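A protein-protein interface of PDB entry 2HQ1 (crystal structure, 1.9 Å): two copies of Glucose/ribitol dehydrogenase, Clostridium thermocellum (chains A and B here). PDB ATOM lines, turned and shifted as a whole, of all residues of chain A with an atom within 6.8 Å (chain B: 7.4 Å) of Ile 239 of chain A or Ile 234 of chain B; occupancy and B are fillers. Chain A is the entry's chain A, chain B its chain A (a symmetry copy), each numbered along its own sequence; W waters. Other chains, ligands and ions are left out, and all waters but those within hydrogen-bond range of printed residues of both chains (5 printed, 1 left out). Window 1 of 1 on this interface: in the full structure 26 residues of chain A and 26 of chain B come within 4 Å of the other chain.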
ATOM      1  N   ASN A 181      -4.256 -18.803  29.764  1.00  0.00           N
ATOM      2  CA  ASN A 181      -3.050 -18.035  29.436  1.00  0.00           C
ATOM      3  C   ASN A 181      -3.230 -17.323  28.113  1.00  0.00           C
ATOM      4  O   ASN A 181      -4.194 -17.603  27.379  1.00  0.00           O
ATOM      5  CB  ASN A 181      -1.806 -18.931  29.389  1.00  0.00           C
ATOM      6  CG  ASN A 181      -1.426 -19.483  30.744  1.00  0.00           C
ATOM      7  OD1 ASN A 181      -0.981 -18.753  31.625  1.00  0.00           O
ATOM      8  ND2 ASN A 181      -1.576 -20.787  30.904  1.00  0.00           N
ATOM      9  N   ALA A 182      -2.320 -16.400  27.814  1.00  0.00           N
ATOM     10  CA  ALA A 182      -2.392 -15.666  26.535  1.00  0.00           C
ATOM     11  C   ALA A 182      -1.078 -15.761  25.754  1.00  0.00           C
ATOM     12  O   ALA A 182       0.002 -15.953  26.336  1.00  0.00           O
ATOM     13  CB  ALA A 182      -2.776 -14.195  26.769  1.00  0.00           C
ATOM     14  N   VAL A 183      -1.192 -15.643  24.432  1.00  0.00           N
ATOM     15  CA  VAL A 183      -0.035 -15.527  23.549  1.00  0.00           C
ATOM     16  C   VAL A 183      -0.152 -14.162  22.852  1.00  0.00           C
ATOM     17  O   VAL A 183      -1.192 -13.845  22.275  1.00  0.00           O
ATOM     18  CB  VAL A 183       0.043 -16.688  22.521  1.00  0.00           C
ATOM     19  CG1 VAL A 183       1.238 -16.492  21.581  1.00  0.00           C
ATOM     20  CG2 VAL A 183       0.175 -18.057  23.218  1.00  0.00           C
ATOM     21  N   ALA A 184       0.897 -13.348  22.943  1.00  0.00           N
ATOM     22  CA  ALA A 184       0.903 -12.034  22.322  1.00  0.00           C
ATOM     23  C   ALA A 184       1.969 -11.963  21.227  1.00  0.00           C
ATOM     24  O   ALA A 184       3.139 -11.735  21.512  1.00  0.00           O
ATOM     25  CB  ALA A 184       1.107 -10.925  23.383  1.00  0.00           C
ATOM     26  N   PRO A 185       1.566 -12.207  19.968  1.00  0.00           N
ATOM     27  CA  PRO A 185       2.508 -12.114  18.863  1.00  0.00           C
ATOM     28  C   PRO A 185       2.865 -10.669  18.504  1.00  0.00           C
ATOM     29  O   PRO A 185       2.011  -9.780  18.553  1.00  0.00           O
ATOM     30  CB  PRO A 185       1.754 -12.777  17.695  1.00  0.00           C
ATOM     31  CG  PRO A 185       0.557 -13.453  18.312  1.00  0.00           C
ATOM     32  CD  PRO A 185       0.233 -12.621  19.509  1.00  0.00           C
ATOM     33  N   LEU A 210      15.472  -9.123  17.115  1.00  0.00           N
ATOM     34  CA  LEU A 210      15.860 -10.330  16.376  1.00  0.00           C
ATOM     35  C   LEU A 210      16.018 -10.087  14.870  1.00  0.00           C
ATOM     36  O   LEU A 210      16.541 -10.942  14.161  1.00  0.00           O
ATOM     37  CB  LEU A 210      14.910 -11.506  16.646  1.00  0.00           C
ATOM     38  CG  LEU A 210      15.062 -12.272  17.971  1.00  0.00           C
ATOM     39  CD1 LEU A 210      14.117 -13.462  17.985  1.00  0.00           C
ATOM     40  CD2 LEU A 210      16.492 -12.734  18.235  1.00  0.00           C
ATOM     41  N   GLU A 218       5.622 -20.620  14.389  1.00  0.00           N
ATOM     42  CA  GLU A 218       6.199 -20.272  15.699  1.00  0.00           C
ATOM     43  C   GLU A 218       5.104 -19.967  16.722  1.00  0.00           C
ATOM     44  O   GLU A 218       5.144 -20.484  17.842  1.00  0.00           O
ATOM     45  CB  GLU A 218       7.166 -19.089  15.576  1.00  0.00           C
ATOM     46  CG  GLU A 218       8.516 -19.453  14.975  1.00  0.00           C
ATOM     47  CD  GLU A 218       9.291 -18.251  14.439  1.00  0.00           C
ATOM     48  OE1 GLU A 218      10.462 -18.436  14.057  1.00  0.00           O
ATOM     49  OE2 GLU A 218       8.747 -17.133  14.405  1.00  0.00           O
ATOM     50  N   VAL A 222       3.980 -22.240  20.161  1.00  0.00           N
ATOM     51  CA  VAL A 222       3.783 -21.716  21.510  1.00  0.00           C
ATOM     52  C   VAL A 222       2.399 -22.125  22.044  1.00  0.00           C
ATOM     53  O   VAL A 222       2.270 -22.524  23.213  1.00  0.00           O
ATOM     54  CB  VAL A 222       3.961 -20.189  21.601  1.00  0.00           C
ATOM     55  CG1 VAL A 222       3.682 -19.700  23.024  1.00  0.00           C
ATOM     56  CG2 VAL A 222       5.386 -19.770  21.183  1.00  0.00           C
ATOM     57  N   PHE A 225       2.679 -25.713  23.087  1.00  0.00           N
ATOM     58  CA  PHE A 225       3.219 -25.733  24.458  1.00  0.00           C
ATOM     59  C   PHE A 225       2.138 -25.451  25.512  1.00  0.00           C
ATOM     60  O   PHE A 225       1.957 -26.240  26.442  1.00  0.00           O
ATOM     61  CB  PHE A 225       4.379 -24.733  24.589  1.00  0.00           C
ATOM     62  CG  PHE A 225       4.821 -24.485  26.015  1.00  0.00           C
ATOM     63  CD1 PHE A 225       5.467 -25.479  26.744  1.00  0.00           C
ATOM     64  CD2 PHE A 225       4.570 -23.262  26.627  1.00  0.00           C
ATOM     65  CE1 PHE A 225       5.866 -25.254  28.062  1.00  0.00           C
ATOM     66  CE2 PHE A 225       4.970 -23.022  27.949  1.00  0.00           C
ATOM     67  CZ  PHE A 225       5.616 -24.019  28.670  1.00  0.00           C
ATOM     68  N   LEU A 226       1.406 -24.350  25.347  1.00  0.00           N
ATOM     69  CA  LEU A 226       0.313 -24.015  26.272  1.00  0.00           C
ATOM     70  C   LEU A 226      -0.850 -25.021  26.301  1.00  0.00           C
ATOM     71  O   LEU A 226      -1.598 -25.059  27.275  1.00  0.00           O
ATOM     72  CB  LEU A 226      -0.218 -22.600  26.030  1.00  0.00           C
ATOM     73  CG  LEU A 226       0.800 -21.500  26.349  1.00  0.00           C
ATOM     74  CD1 LEU A 226       0.238 -20.143  25.908  1.00  0.00           C
ATOM     75  CD2 LEU A 226       1.194 -21.493  27.841  1.00  0.00           C
ATOM     76  N   SER A 231       3.220 -27.351  29.923  1.00  0.00           N
ATOM     77  CA  SER A 231       2.912 -26.052  30.509  1.00  0.00           C
ATOM     78  C   SER A 231       2.048 -26.163  31.770  1.00  0.00           C
ATOM     79  O   SER A 231       1.510 -25.171  32.239  1.00  0.00           O
ATOM     80  CB  SER A 231       2.198 -25.166  29.479  1.00  0.00           C
ATOM     81  OG  SER A 231       0.994 -25.785  29.063  1.00  0.00           O
ATOM     82  N   ILE A 234       1.346 -23.487  34.879  1.00  0.00           N
ATOM     83  CA  ILE A 234       1.419 -22.109  34.388  1.00  0.00           C
ATOM     84  C   ILE A 234       0.003 -21.609  34.151  1.00  0.00           C
ATOM     85  O   ILE A 234      -0.731 -22.172  33.340  1.00  0.00           O
ATOM     86  CB  ILE A 234       2.223 -22.006  33.061  1.00  0.00           C
ATOM     87  CG1 ILE A 234       3.650 -22.536  33.238  1.00  0.00           C
ATOM     88  CG2 ILE A 234       2.204 -20.560  32.524  1.00  0.00           C
ATOM     89  CD1 ILE A 234       4.397 -22.749  31.906  1.00  0.00           C
ATOM     90  N   GLN A 237      -0.755 -16.168  32.698  1.00  0.00           N
ATOM     91  CA  GLN A 237       0.471 -15.637  32.122  1.00  0.00           C
ATOM     92  C   GLN A 237       0.291 -15.204  30.667  1.00  0.00           C
ATOM     93  O   GLN A 237      -0.589 -15.702  29.972  1.00  0.00           O
ATOM     94  CB  GLN A 237       1.591 -16.679  32.212  1.00  0.00           C
ATOM     95  CG  GLN A 237       1.902 -17.146  33.649  1.00  0.00           C
ATOM     96  CD  GLN A 237       2.134 -16.009  34.610  1.00  0.00           C
ATOM     97  OE1 GLN A 237       2.936 -15.111  34.348  1.00  0.00           O
ATOM     98  NE2 GLN A 237       1.449 -16.050  35.749  1.00  0.00           N
ATOM     99  N   VAL A 238       1.147 -14.284  30.222  1.00  0.00           N
ATOM    100  CA  VAL A 238       1.220 -13.921  28.804  1.00  0.00           C
ATOM    101  C   VAL A 238       2.598 -14.253  28.242  1.00  0.00           C
ATOM    102  O   VAL A 238       3.616 -13.816  28.787  1.00  0.00           O
ATOM    103  CB  VAL A 238       0.975 -12.408  28.593  1.00  0.00           C
ATOM    104  CG1 VAL A 238       0.896 -12.077  27.092  1.00  0.00           C
ATOM    105  CG2 VAL A 238      -0.281 -11.976  29.273  1.00  0.00           C
ATOM    106  N   ILE A 239       2.630 -15.009  27.149  1.00  0.00           N
ATOM    107  CA  ILE A 239       3.881 -15.266  26.452  1.00  0.00           C
ATOM    108  C   ILE A 239       3.959 -14.352  25.227  1.00  0.00           C
ATOM    109  O   ILE A 239       3.175 -14.492  24.279  1.00  0.00           O
ATOM    110  CB  ILE A 239       4.038 -16.763  26.061  1.00  0.00           C
ATOM    111  CG1 ILE A 239       4.097 -17.628  27.340  1.00  0.00           C
ATOM    112  CG2 ILE A 239       5.287 -16.973  25.185  1.00  0.00           C
ATOM    113  CD1 ILE A 239       4.032 -19.132  27.097  1.00  0.00           C
ATOM    114  N   ASN A 240       4.894 -13.403  25.288  1.00  0.00           N
ATOM    115  CA  ASN A 240       5.182 -12.514  24.172  1.00  0.00           C
ATOM    116  C   ASN A 240       6.115 -13.219  23.190  1.00  0.00           C
ATOM    117  O   ASN A 240       7.213 -13.627  23.553  1.00  0.00           O
ATOM    118  CB  ASN A 240       5.817 -11.220  24.670  1.00  0.00           C
ATOM    119  CG  ASN A 240       4.943 -10.475  25.653  1.00  0.00           C
ATOM    120  OD1 ASN A 240       3.876  -9.985  25.304  1.00  0.00           O
ATOM    121  ND2 ASN A 240       5.409 -10.362  26.890  1.00  0.00           N
ATOM    122  N   ILE A 241       5.651 -13.386  21.960  1.00  0.00           N
ATOM    123  CA  ILE A 241       6.468 -13.941  20.886  1.00  0.00           C
ATOM    124  C   ILE A 241       6.624 -12.842  19.827  1.00  0.00           C
ATOM    125  O   ILE A 241       5.838 -12.721  18.885  1.00  0.00           O
ATOM    126  CB  ILE A 241       5.908 -15.313  20.360  1.00  0.00           C
ATOM    127  CG1 ILE A 241       6.778 -15.871  19.218  1.00  0.00           C
ATOM    128  CG2 ILE A 241       4.414 -15.227  19.984  1.00  0.00           C
ATOM    129  CD1 ILE A 241       6.713 -17.381  19.066  1.00  0.00           C
ATOM    130  N   ASP A 242       7.633 -12.008  20.027  1.00  0.00           N
ATOM    131  CA  ASP A 242       7.731 -10.751  19.291  1.00  0.00           C
ATOM    132  C   ASP A 242       9.159 -10.394  18.892  1.00  0.00           C
ATOM    133  O   ASP A 242       9.421  -9.270  18.474  1.00  0.00           O
ATOM    134  CB  ASP A 242       7.125  -9.616  20.124  1.00  0.00           C
ATOM    135  CG  ASP A 242       7.741  -9.505  21.510  1.00  0.00           C
ATOM    136  OD1 ASP A 242       8.920  -9.873  21.705  1.00  0.00           O
ATOM    137  OD2 ASP A 242       7.035  -9.036  22.420  1.00  0.00           O
ATOM    138  N   GLY A 243      10.075 -11.345  19.056  1.00  0.00           N
ATOM    139  CA  GLY A 243      11.479 -11.145  18.711  1.00  0.00           C
ATOM    140  C   GLY A 243      12.176 -10.105  19.564  1.00  0.00           C
ATOM    141  O   GLY A 243      13.148  -9.488  19.128  1.00  0.00           O
ATOM    142  N   GLY A 244      11.672  -9.912  20.782  1.00  0.00           N
ATOM    143  CA  GLY A 244      12.272  -8.984  21.728  1.00  0.00           C
ATOM    144  C   GLY A 244      11.744  -7.571  21.608  1.00  0.00           C
ATOM    145  O   GLY A 244      12.214  -6.675  22.311  1.00  0.00           O
ATOM    146  N   LYS B 136      21.012 -20.564  23.331  1.00  0.00           N
ATOM    147  CA  LYS B 136      19.904 -20.259  24.220  1.00  0.00           C
ATOM    148  C   LYS B 136      20.440 -20.176  25.653  1.00  0.00           C
ATOM    149  O   LYS B 136      21.075 -21.101  26.124  1.00  0.00           O
ATOM    150  CB  LYS B 136      18.833 -21.339  24.092  1.00  0.00           C
ATOM    151  CG  LYS B 136      18.242 -21.494  22.668  1.00  0.00           C
ATOM    152  CD  LYS B 136      16.754 -21.227  22.629  1.00  0.00           C
ATOM    153  CE  LYS B 136      16.141 -21.677  21.311  1.00  0.00           C
ATOM    154  NZ  LYS B 136      14.662 -21.556  21.302  1.00  0.00           N
ATOM    155  N   ALA B 170      19.355 -10.381  26.518  1.00  0.00           N
ATOM    156  CA  ALA B 170      18.508 -10.681  25.366  1.00  0.00           C
ATOM    157  C   ALA B 170      18.612  -9.551  24.331  1.00  0.00           C
ATOM    158  O   ALA B 170      18.853  -9.800  23.149  1.00  0.00           O
ATOM    159  CB  ALA B 170      17.070 -10.863  25.813  1.00  0.00           C
ATOM    160  N   ILE B 178      21.332 -15.054  19.392  1.00  0.00           N
ATOM    161  CA  ILE B 178      21.374 -15.650  20.731  1.00  0.00           C
ATOM    162  C   ILE B 178      20.180 -15.197  21.564  1.00  0.00           C
ATOM    163  O   ILE B 178      19.883 -14.003  21.658  1.00  0.00           O
ATOM    164  CB  ILE B 178      22.707 -15.339  21.447  1.00  0.00           C
ATOM    165  CG1 ILE B 178      23.882 -15.878  20.618  1.00  0.00           C
ATOM    166  CG2 ILE B 178      22.740 -15.911  22.885  1.00  0.00           C
ATOM    167  CD1 ILE B 178      25.196 -15.175  20.874  1.00  0.00           C
ATOM    168  N   TYR B 179      19.509 -16.179  22.164  1.00  0.00           N
ATOM    169  CA  TYR B 179      18.312 -15.983  22.978  1.00  0.00           C
ATOM    170  C   TYR B 179      18.682 -15.911  24.459  1.00  0.00           C
ATOM    171  O   TYR B 179      19.638 -16.563  24.897  1.00  0.00           O
ATOM    172  CB  TYR B 179      17.375 -17.183  22.793  1.00  0.00           C
ATOM    173  CG  TYR B 179      16.722 -17.311  21.438  1.00  0.00           C
ATOM    174  CD1 TYR B 179      17.216 -18.182  20.479  1.00  0.00           C
ATOM    175  CD2 TYR B 179      15.585 -16.569  21.132  1.00  0.00           C
ATOM    176  CE1 TYR B 179      16.593 -18.303  19.225  1.00  0.00           C
ATOM    177  CE2 TYR B 179      14.963 -16.676  19.905  1.00  0.00           C
ATOM    178  CZ  TYR B 179      15.466 -17.542  18.955  1.00  0.00           C
ATOM    179  OH  TYR B 179      14.813 -17.641  17.753  1.00  0.00           O
ATOM    180  N   CYS B 180      17.931 -15.113  25.215  1.00  0.00           N
ATOM    181  CA  CYS B 180      18.011 -15.144  26.670  1.00  0.00           C
ATOM    182  C   CYS B 180      16.625 -15.010  27.277  1.00  0.00           C
ATOM    183  O   CYS B 180      15.922 -14.020  27.048  1.00  0.00           O
ATOM    184  CB  CYS B 180      18.939 -14.061  27.227  1.00  0.00           C
ATOM    185  SG  CYS B 180      19.296 -14.300  28.998  1.00  0.00           S
ATOM    186  N   ASN B 181      16.229 -16.017  28.057  1.00  0.00           N
ATOM    187  CA  ASN B 181      14.941 -15.958  28.757  1.00  0.00           C
ATOM    188  C   ASN B 181      15.099 -16.448  30.180  1.00  0.00           C
ATOM    189  O   ASN B 181      16.147 -17.019  30.531  1.00  0.00           O
ATOM    190  CB  ASN B 181      13.866 -16.777  28.032  1.00  0.00           C
ATOM    191  CG  ASN B 181      13.482 -16.191  26.693  1.00  0.00           C
ATOM    192  OD1 ASN B 181      12.862 -15.135  26.615  1.00  0.00           O
ATOM    193  ND2 ASN B 181      13.831 -16.895  25.629  1.00  0.00           N
ATOM    194  N   PHE B 225      11.015 -26.592  26.863  1.00  0.00           N
ATOM    195  CA  PHE B 225      10.388 -25.675  25.896  1.00  0.00           C
ATOM    196  C   PHE B 225      11.328 -24.533  25.483  1.00  0.00           C
ATOM    197  O   PHE B 225      11.567 -24.325  24.291  1.00  0.00           O
ATOM    198  CB  PHE B 225       9.073 -25.116  26.467  1.00  0.00           C
ATOM    199  CG  PHE B 225       8.494 -23.968  25.670  1.00  0.00           C
ATOM    200  CD1 PHE B 225       7.967 -24.177  24.398  1.00  0.00           C
ATOM    201  CD2 PHE B 225       8.498 -22.678  26.188  1.00  0.00           C
ATOM    202  CE1 PHE B 225       7.441 -23.117  23.659  1.00  0.00           C
ATOM    203  CE2 PHE B 225       7.968 -21.605  25.458  1.00  0.00           C
ATOM    204  CZ  PHE B 225       7.442 -21.823  24.190  1.00  0.00           C
ATOM    205  N   LEU B 226      11.881 -23.821  26.464  1.00  0.00           N
ATOM    206  CA  LEU B 226      12.835 -22.739  26.177  1.00  0.00           C
ATOM    207  C   LEU B 226      14.141 -23.182  25.495  1.00  0.00           C
ATOM    208  O   LEU B 226      14.811 -22.362  24.874  1.00  0.00           O
ATOM    209  CB  LEU B 226      13.145 -21.913  27.427  1.00  0.00           C
ATOM    210  CG  LEU B 226      11.941 -21.127  27.958  1.00  0.00           C
ATOM    211  CD1 LEU B 226      12.306 -20.481  29.300  1.00  0.00           C
ATOM    212  CD2 LEU B 226      11.444 -20.078  26.940  1.00  0.00           C
ATOM    213  N   ASP B 230      10.653 -24.979  19.581  1.00  0.00           N
ATOM    214  CA  ASP B 230       9.272 -24.547  19.854  1.00  0.00           C
ATOM    215  C   ASP B 230       9.165 -23.143  20.449  1.00  0.00           C
ATOM    216  O   ASP B 230       8.111 -22.523  20.371  1.00  0.00           O
ATOM    217  CB  ASP B 230       8.562 -25.539  20.782  1.00  0.00           C
ATOM    218  CG  ASP B 230       8.275 -26.861  20.112  1.00  0.00           C
ATOM    219  OD1 ASP B 230       8.321 -26.940  18.868  1.00  0.00           O
ATOM    220  OD2 ASP B 230       7.982 -27.831  20.836  1.00  0.00           O
ATOM    221  N   SER B 231      10.249 -22.667  21.056  1.00  0.00           N
ATOM    222  CA  SER B 231      10.299 -21.338  21.653  1.00  0.00           C
ATOM    223  C   SER B 231      11.075 -20.333  20.795  1.00  0.00           C
ATOM    224  O   SER B 231      11.409 -19.253  21.259  1.00  0.00           O
ATOM    225  CB  SER B 231      10.933 -21.411  23.049  1.00  0.00           C
ATOM    226  OG  SER B 231      12.248 -21.927  22.955  1.00  0.00           O
ATOM    227  N   ASN B 232      11.385 -20.693  19.549  1.00  0.00           N
ATOM    228  CA  ASN B 232      12.004 -19.727  18.629  1.00  0.00           C
ATOM    229  C   ASN B 232      11.198 -18.444  18.521  1.00  0.00           C
ATOM    230  O   ASN B 232       9.964 -18.457  18.575  1.00  0.00           O
ATOM    231  CB  ASN B 232      12.238 -20.342  17.245  1.00  0.00           C
ATOM    232  CG  ASN B 232      13.340 -21.379  17.253  1.00  0.00           C
ATOM    233  OD1 ASN B 232      14.062 -21.532  18.246  1.00  0.00           O
ATOM    234  ND2 ASN B 232      13.483 -22.099  16.140  1.00  0.00           N
ATOM    235  N   TYR B 233      11.920 -17.338  18.396  1.00  0.00           N
ATOM    236  CA  TYR B 233      11.357 -15.998  18.336  1.00  0.00           C
ATOM    237  C   TYR B 233      10.919 -15.416  19.686  1.00  0.00           C
ATOM    238  O   TYR B 233      10.427 -14.290  19.743  1.00  0.00           O
ATOM    239  CB  TYR B 233      10.219 -15.927  17.314  1.00  0.00           C
ATOM    240  CG  TYR B 233      10.044 -14.569  16.700  1.00  0.00           C
ATOM    241  CD1 TYR B 233       8.842 -13.874  16.836  1.00  0.00           C
ATOM    242  CD2 TYR B 233      11.079 -13.968  15.988  1.00  0.00           C
ATOM    243  CE1 TYR B 233       8.663 -12.622  16.262  1.00  0.00           C
ATOM    244  CE2 TYR B 233      10.912 -12.707  15.403  1.00  0.00           C
ATOM    245  CZ  TYR B 233       9.703 -12.045  15.548  1.00  0.00           C
ATOM    246  OH  TYR B 233       9.517 -10.808  14.990  1.00  0.00           O
ATOM    247  N   ILE B 234      11.103 -16.172  20.764  1.00  0.00           N
ATOM    248  CA  ILE B 234      10.843 -15.653  22.108  1.00  0.00           C
ATOM    249  C   ILE B 234      12.173 -15.274  22.741  1.00  0.00           C
ATOM    250  O   ILE B 234      13.046 -16.123  22.917  1.00  0.00           O
ATOM    251  CB  ILE B 234      10.132 -16.702  23.009  1.00  0.00           C
ATOM    252  CG1 ILE B 234       8.802 -17.147  22.394  1.00  0.00           C
ATOM    253  CG2 ILE B 234       9.956 -16.158  24.442  1.00  0.00           C
ATOM    254  CD1 ILE B 234       8.198 -18.396  23.067  1.00  0.00           C
ATOM    255  N   THR B 235      12.327 -14.001  23.078  1.00  0.00           N
ATOM    256  CA  THR B 235      13.512 -13.559  23.801  1.00  0.00           C
ATOM    257  C   THR B 235      13.225 -12.413  24.756  1.00  0.00           C
ATOM    258  O   THR B 235      12.298 -11.622  24.536  1.00  0.00           O
ATOM    259  CB  THR B 235      14.681 -13.228  22.840  1.00  0.00           C
ATOM    260  OG1 THR B 235      15.908 -13.353  23.557  1.00  0.00           O
ATOM    261  CG2 THR B 235      14.539 -11.808  22.248  1.00  0.00           C
ATOM    262  N   GLY B 236      14.010 -12.346  25.831  1.00  0.00           N
ATOM    263  CA  GLY B 236      13.857 -11.303  26.837  1.00  0.00           C
ATOM    264  C   GLY B 236      12.621 -11.459  27.695  1.00  0.00           C
ATOM    265  O   GLY B 236      12.134 -10.487  28.274  1.00  0.00           O
ATOM    266  N   GLN B 237      12.141 -12.696  27.805  1.00  0.00           N
ATOM    267  CA  GLN B 237      10.891 -12.977  28.493  1.00  0.00           C
ATOM    268  C   GLN B 237      11.104 -13.747  29.796  1.00  0.00           C
ATOM    269  O   GLN B 237      12.101 -14.444  29.953  1.00  0.00           O
ATOM    270  CB  GLN B 237       9.951 -13.769  27.577  1.00  0.00           C
ATOM    271  CG  GLN B 237       9.616 -13.056  26.251  1.00  0.00           C
ATOM    272  CD  GLN B 237       9.133 -11.641  26.438  1.00  0.00           C
ATOM    273  OE1 GLN B 237       8.216 -11.383  27.222  1.00  0.00           O
ATOM    274  NE2 GLN B 237       9.730 -10.711  25.700  1.00  0.00           N
ATOM    275  N   VAL B 238      10.145 -13.619  30.713  1.00  0.00           N
ATOM    276  CA  VAL B 238      10.117 -14.447  31.921  1.00  0.00           C
ATOM    277  C   VAL B 238       8.857 -15.305  31.948  1.00  0.00           C
ATOM    278  O   VAL B 238       7.743 -14.781  31.835  1.00  0.00           O
ATOM    279  CB  VAL B 238      10.128 -13.582  33.203  1.00  0.00           C
ATOM    280  CG1 VAL B 238      10.262 -14.469  34.454  1.00  0.00           C
ATOM    281  CG2 VAL B 238      11.244 -12.592  33.163  1.00  0.00           C
ATOM    282  N   ILE B 239       9.028 -16.612  32.112  1.00  0.00           N
ATOM    283  CA  ILE B 239       7.889 -17.501  32.293  1.00  0.00           C
ATOM    284  C   ILE B 239       7.753 -17.829  33.782  1.00  0.00           C
ATOM    285  O   ILE B 239       8.617 -18.497  34.366  1.00  0.00           O
ATOM    286  CB  ILE B 239       8.007 -18.789  31.431  1.00  0.00           C
ATOM    287  CG1 ILE B 239       7.995 -18.411  29.933  1.00  0.00           C
ATOM    288  CG2 ILE B 239       6.876 -19.779  31.766  1.00  0.00           C
ATOM    289  CD1 ILE B 239       8.321 -19.558  28.982  1.00  0.00           C
HETATM  290  O   HOH W   1       6.481 -13.221  27.750  1.00  0.00           O
HETATM  291  O   HOH W   2       4.904 -15.631  32.758  1.00  0.00           O
HETATM  292  O   HOH W   3       7.950  -9.027  16.285  1.00  0.00           O
HETATM  293  O   HOH W   4      11.810 -21.392  14.031  1.00  0.00           O
HETATM  294  O   HOH W   5       9.416 -12.559  22.732  1.00  0.00           O
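N of Gly 243 of chain A sits at hydrogen-bond distance from O of Tyr 233 of chain B, 3.0 Å away. The side-chain amide nitrogen (ND2) of Asn 240 of chain A lies within hydrogen-bond range of the side-chain amide oxygen (OE1) of Gln 237 of chain B (3.0 Å).
Among the printed residues, pairs that only touch across the chains: Ile 241 of chain A with Asn 232 of chain B (3.5 Å), Glu 218 of chain A with Tyr 233 of chain B (3.5 Å), Asp 242 of chain A with Tyr 233 of chain B (3.5 Å), Phe 225 of chain A with Phe 225 of chain B (3.5 Å), Val 222 of chain A with Ile 234 of chain B (3.7 Å), Gly 244 of chain A with Thr 235 of chain B (3.7 Å), Leu 210 of chain A with Tyr 233 of chain B (3.7 Å), Ile 241 of chain A with Tyr 233 of chain B (3.7 Å), Asn 240 of chain A with Ile 234 of chain B (3.8 Å), Leu 210 of chain A with Tyr 179 of chain B (3.8 Å), Ile 239 of chain A with Ile 234 of chain B (3.9 Å), Ile 234 of chain A with Ile 239 of chain B (3.9 Å), Ile 241 of chain A with Ile 234 of chain B (3.9 Å), Val 222 of chain A with Asp 230 of chain B (3.96 Å) and Gly 243 of chain A with Thr 235 of chain B (3.96 Å).
Of the 20 printed residues of chain A, 11 touch a printed residue of chain B. Printed residues of chain A that touch a printed residue of chain B: Leu 210, Glu 218, Val 222, Phe 225, Ile 234, Ile 239, Asn 240, Ile 241, Asp 242, Gly 243 and Gly 244. Hydrophobic or aromatic side chains of chain A within 4 Å of the printed part of chain B: Leu 210, Val 222, Phe 225, Ile 234, Ile 239 and Ile 241. Among the printed residues, no Asp or Glu carboxylate lies within 4 Å of a Lys or Arg side-chain nitrogen of the other chain.
The side-chain carboxylate (OD1) of Asp 242 of chain A is in hydrogen-bond range of the backbone NH (N) of Gly 244 of chain A, 2.9 Å away. The side-chain hydroxyl (OH) of Tyr 179 of chain B is in hydrogen-bond range of the backbone NH (N) of Tyr 233 of chain B (3.0 Å). The side-chain amide oxygen (OD1) of Asn 232 of chain B lies within hydrogen-bond range of the side-chain amino group (NZ) of Lys 136 of chain B, at 3.1 Å. The backbone carbonyl oxygen (O) of Phe 225 of chain B lies within hydrogen-bond range of the side-chain hydroxyl (OG) of Ser 231 of chain B, 2.8 Å away. ND2 of Asn 181 of chain A is in hydrogen-bond range of O of Ile 234 of chain A (2.9 Å). O of Ala 182 of chain A sits at hydrogen-bond distance from N of Ile 239 of chain A, 2.9 Å away.
Phe 225 of chain B touches its own counterpart, Phe 225 of chain A. Ile 234 of chain A touches Ile 239 of chain B, and with the chains exchanged Ile 239 of chain A touches Ile 234 of chain B. 8 positions are printed for both chains. Of the 17 pairs that touch across the chains among the printed residues, 3 have their exchanged pair printed and touching as well.
Of chain B, only Ile 234 (3.9 Å) comes within 4 Å of Ile 239 of chain A. Printed residues of chain B within 4 Å of Asn 240 of chain A: Ile 234 and Gln 237. Of chain A, only Val 222, Ile 239, Asn 240 and Ile 241 come within 4 Å of Ile 234 of chain B. Of the printed residues of chain A, Ile 239 of chain B touches Ile 234 (3.9 Å). The nearest residue of chain B that does not touch Ile 239 of chain A is Ile 239 of chain B (4.7 Å).
Water W1 lies within hydrogen-bond range of the side-chain amide oxygen of Gln 237 of chain B (2.6 Å), the backbone NH of Asn 240 of chain A (2.9 Å) and the backbone carbonyl oxygen of Val 238 of chain A (3.1 Å). Water W2 bridges OE1 of Gln 237 of chain A (2.6 Å) and O of Val 238 of chain B (3.1 Å). Water W5 lies within hydrogen-bond range of the backbone carbonyl oxygen of Asn 240 of chain A (2.6 Å), the side-chain carboxylate of Asp 242 of chain A (2.9 Å) and the backbone NH of Thr 235 of chain B (3.3 Å). Water W3 lies within hydrogen-bond range of the backbone carbonyl oxygen (O) of Asp 242 of chain A and the side-chain hydroxyl (OH) of Tyr 233 of chain B. Water W4 lies within hydrogen-bond range of the side-chain amide nitrogen of Asn 232 of chain B (2.8 Å) and the side-chain carboxylate of Glu 218 of chain A (3.2 Å).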
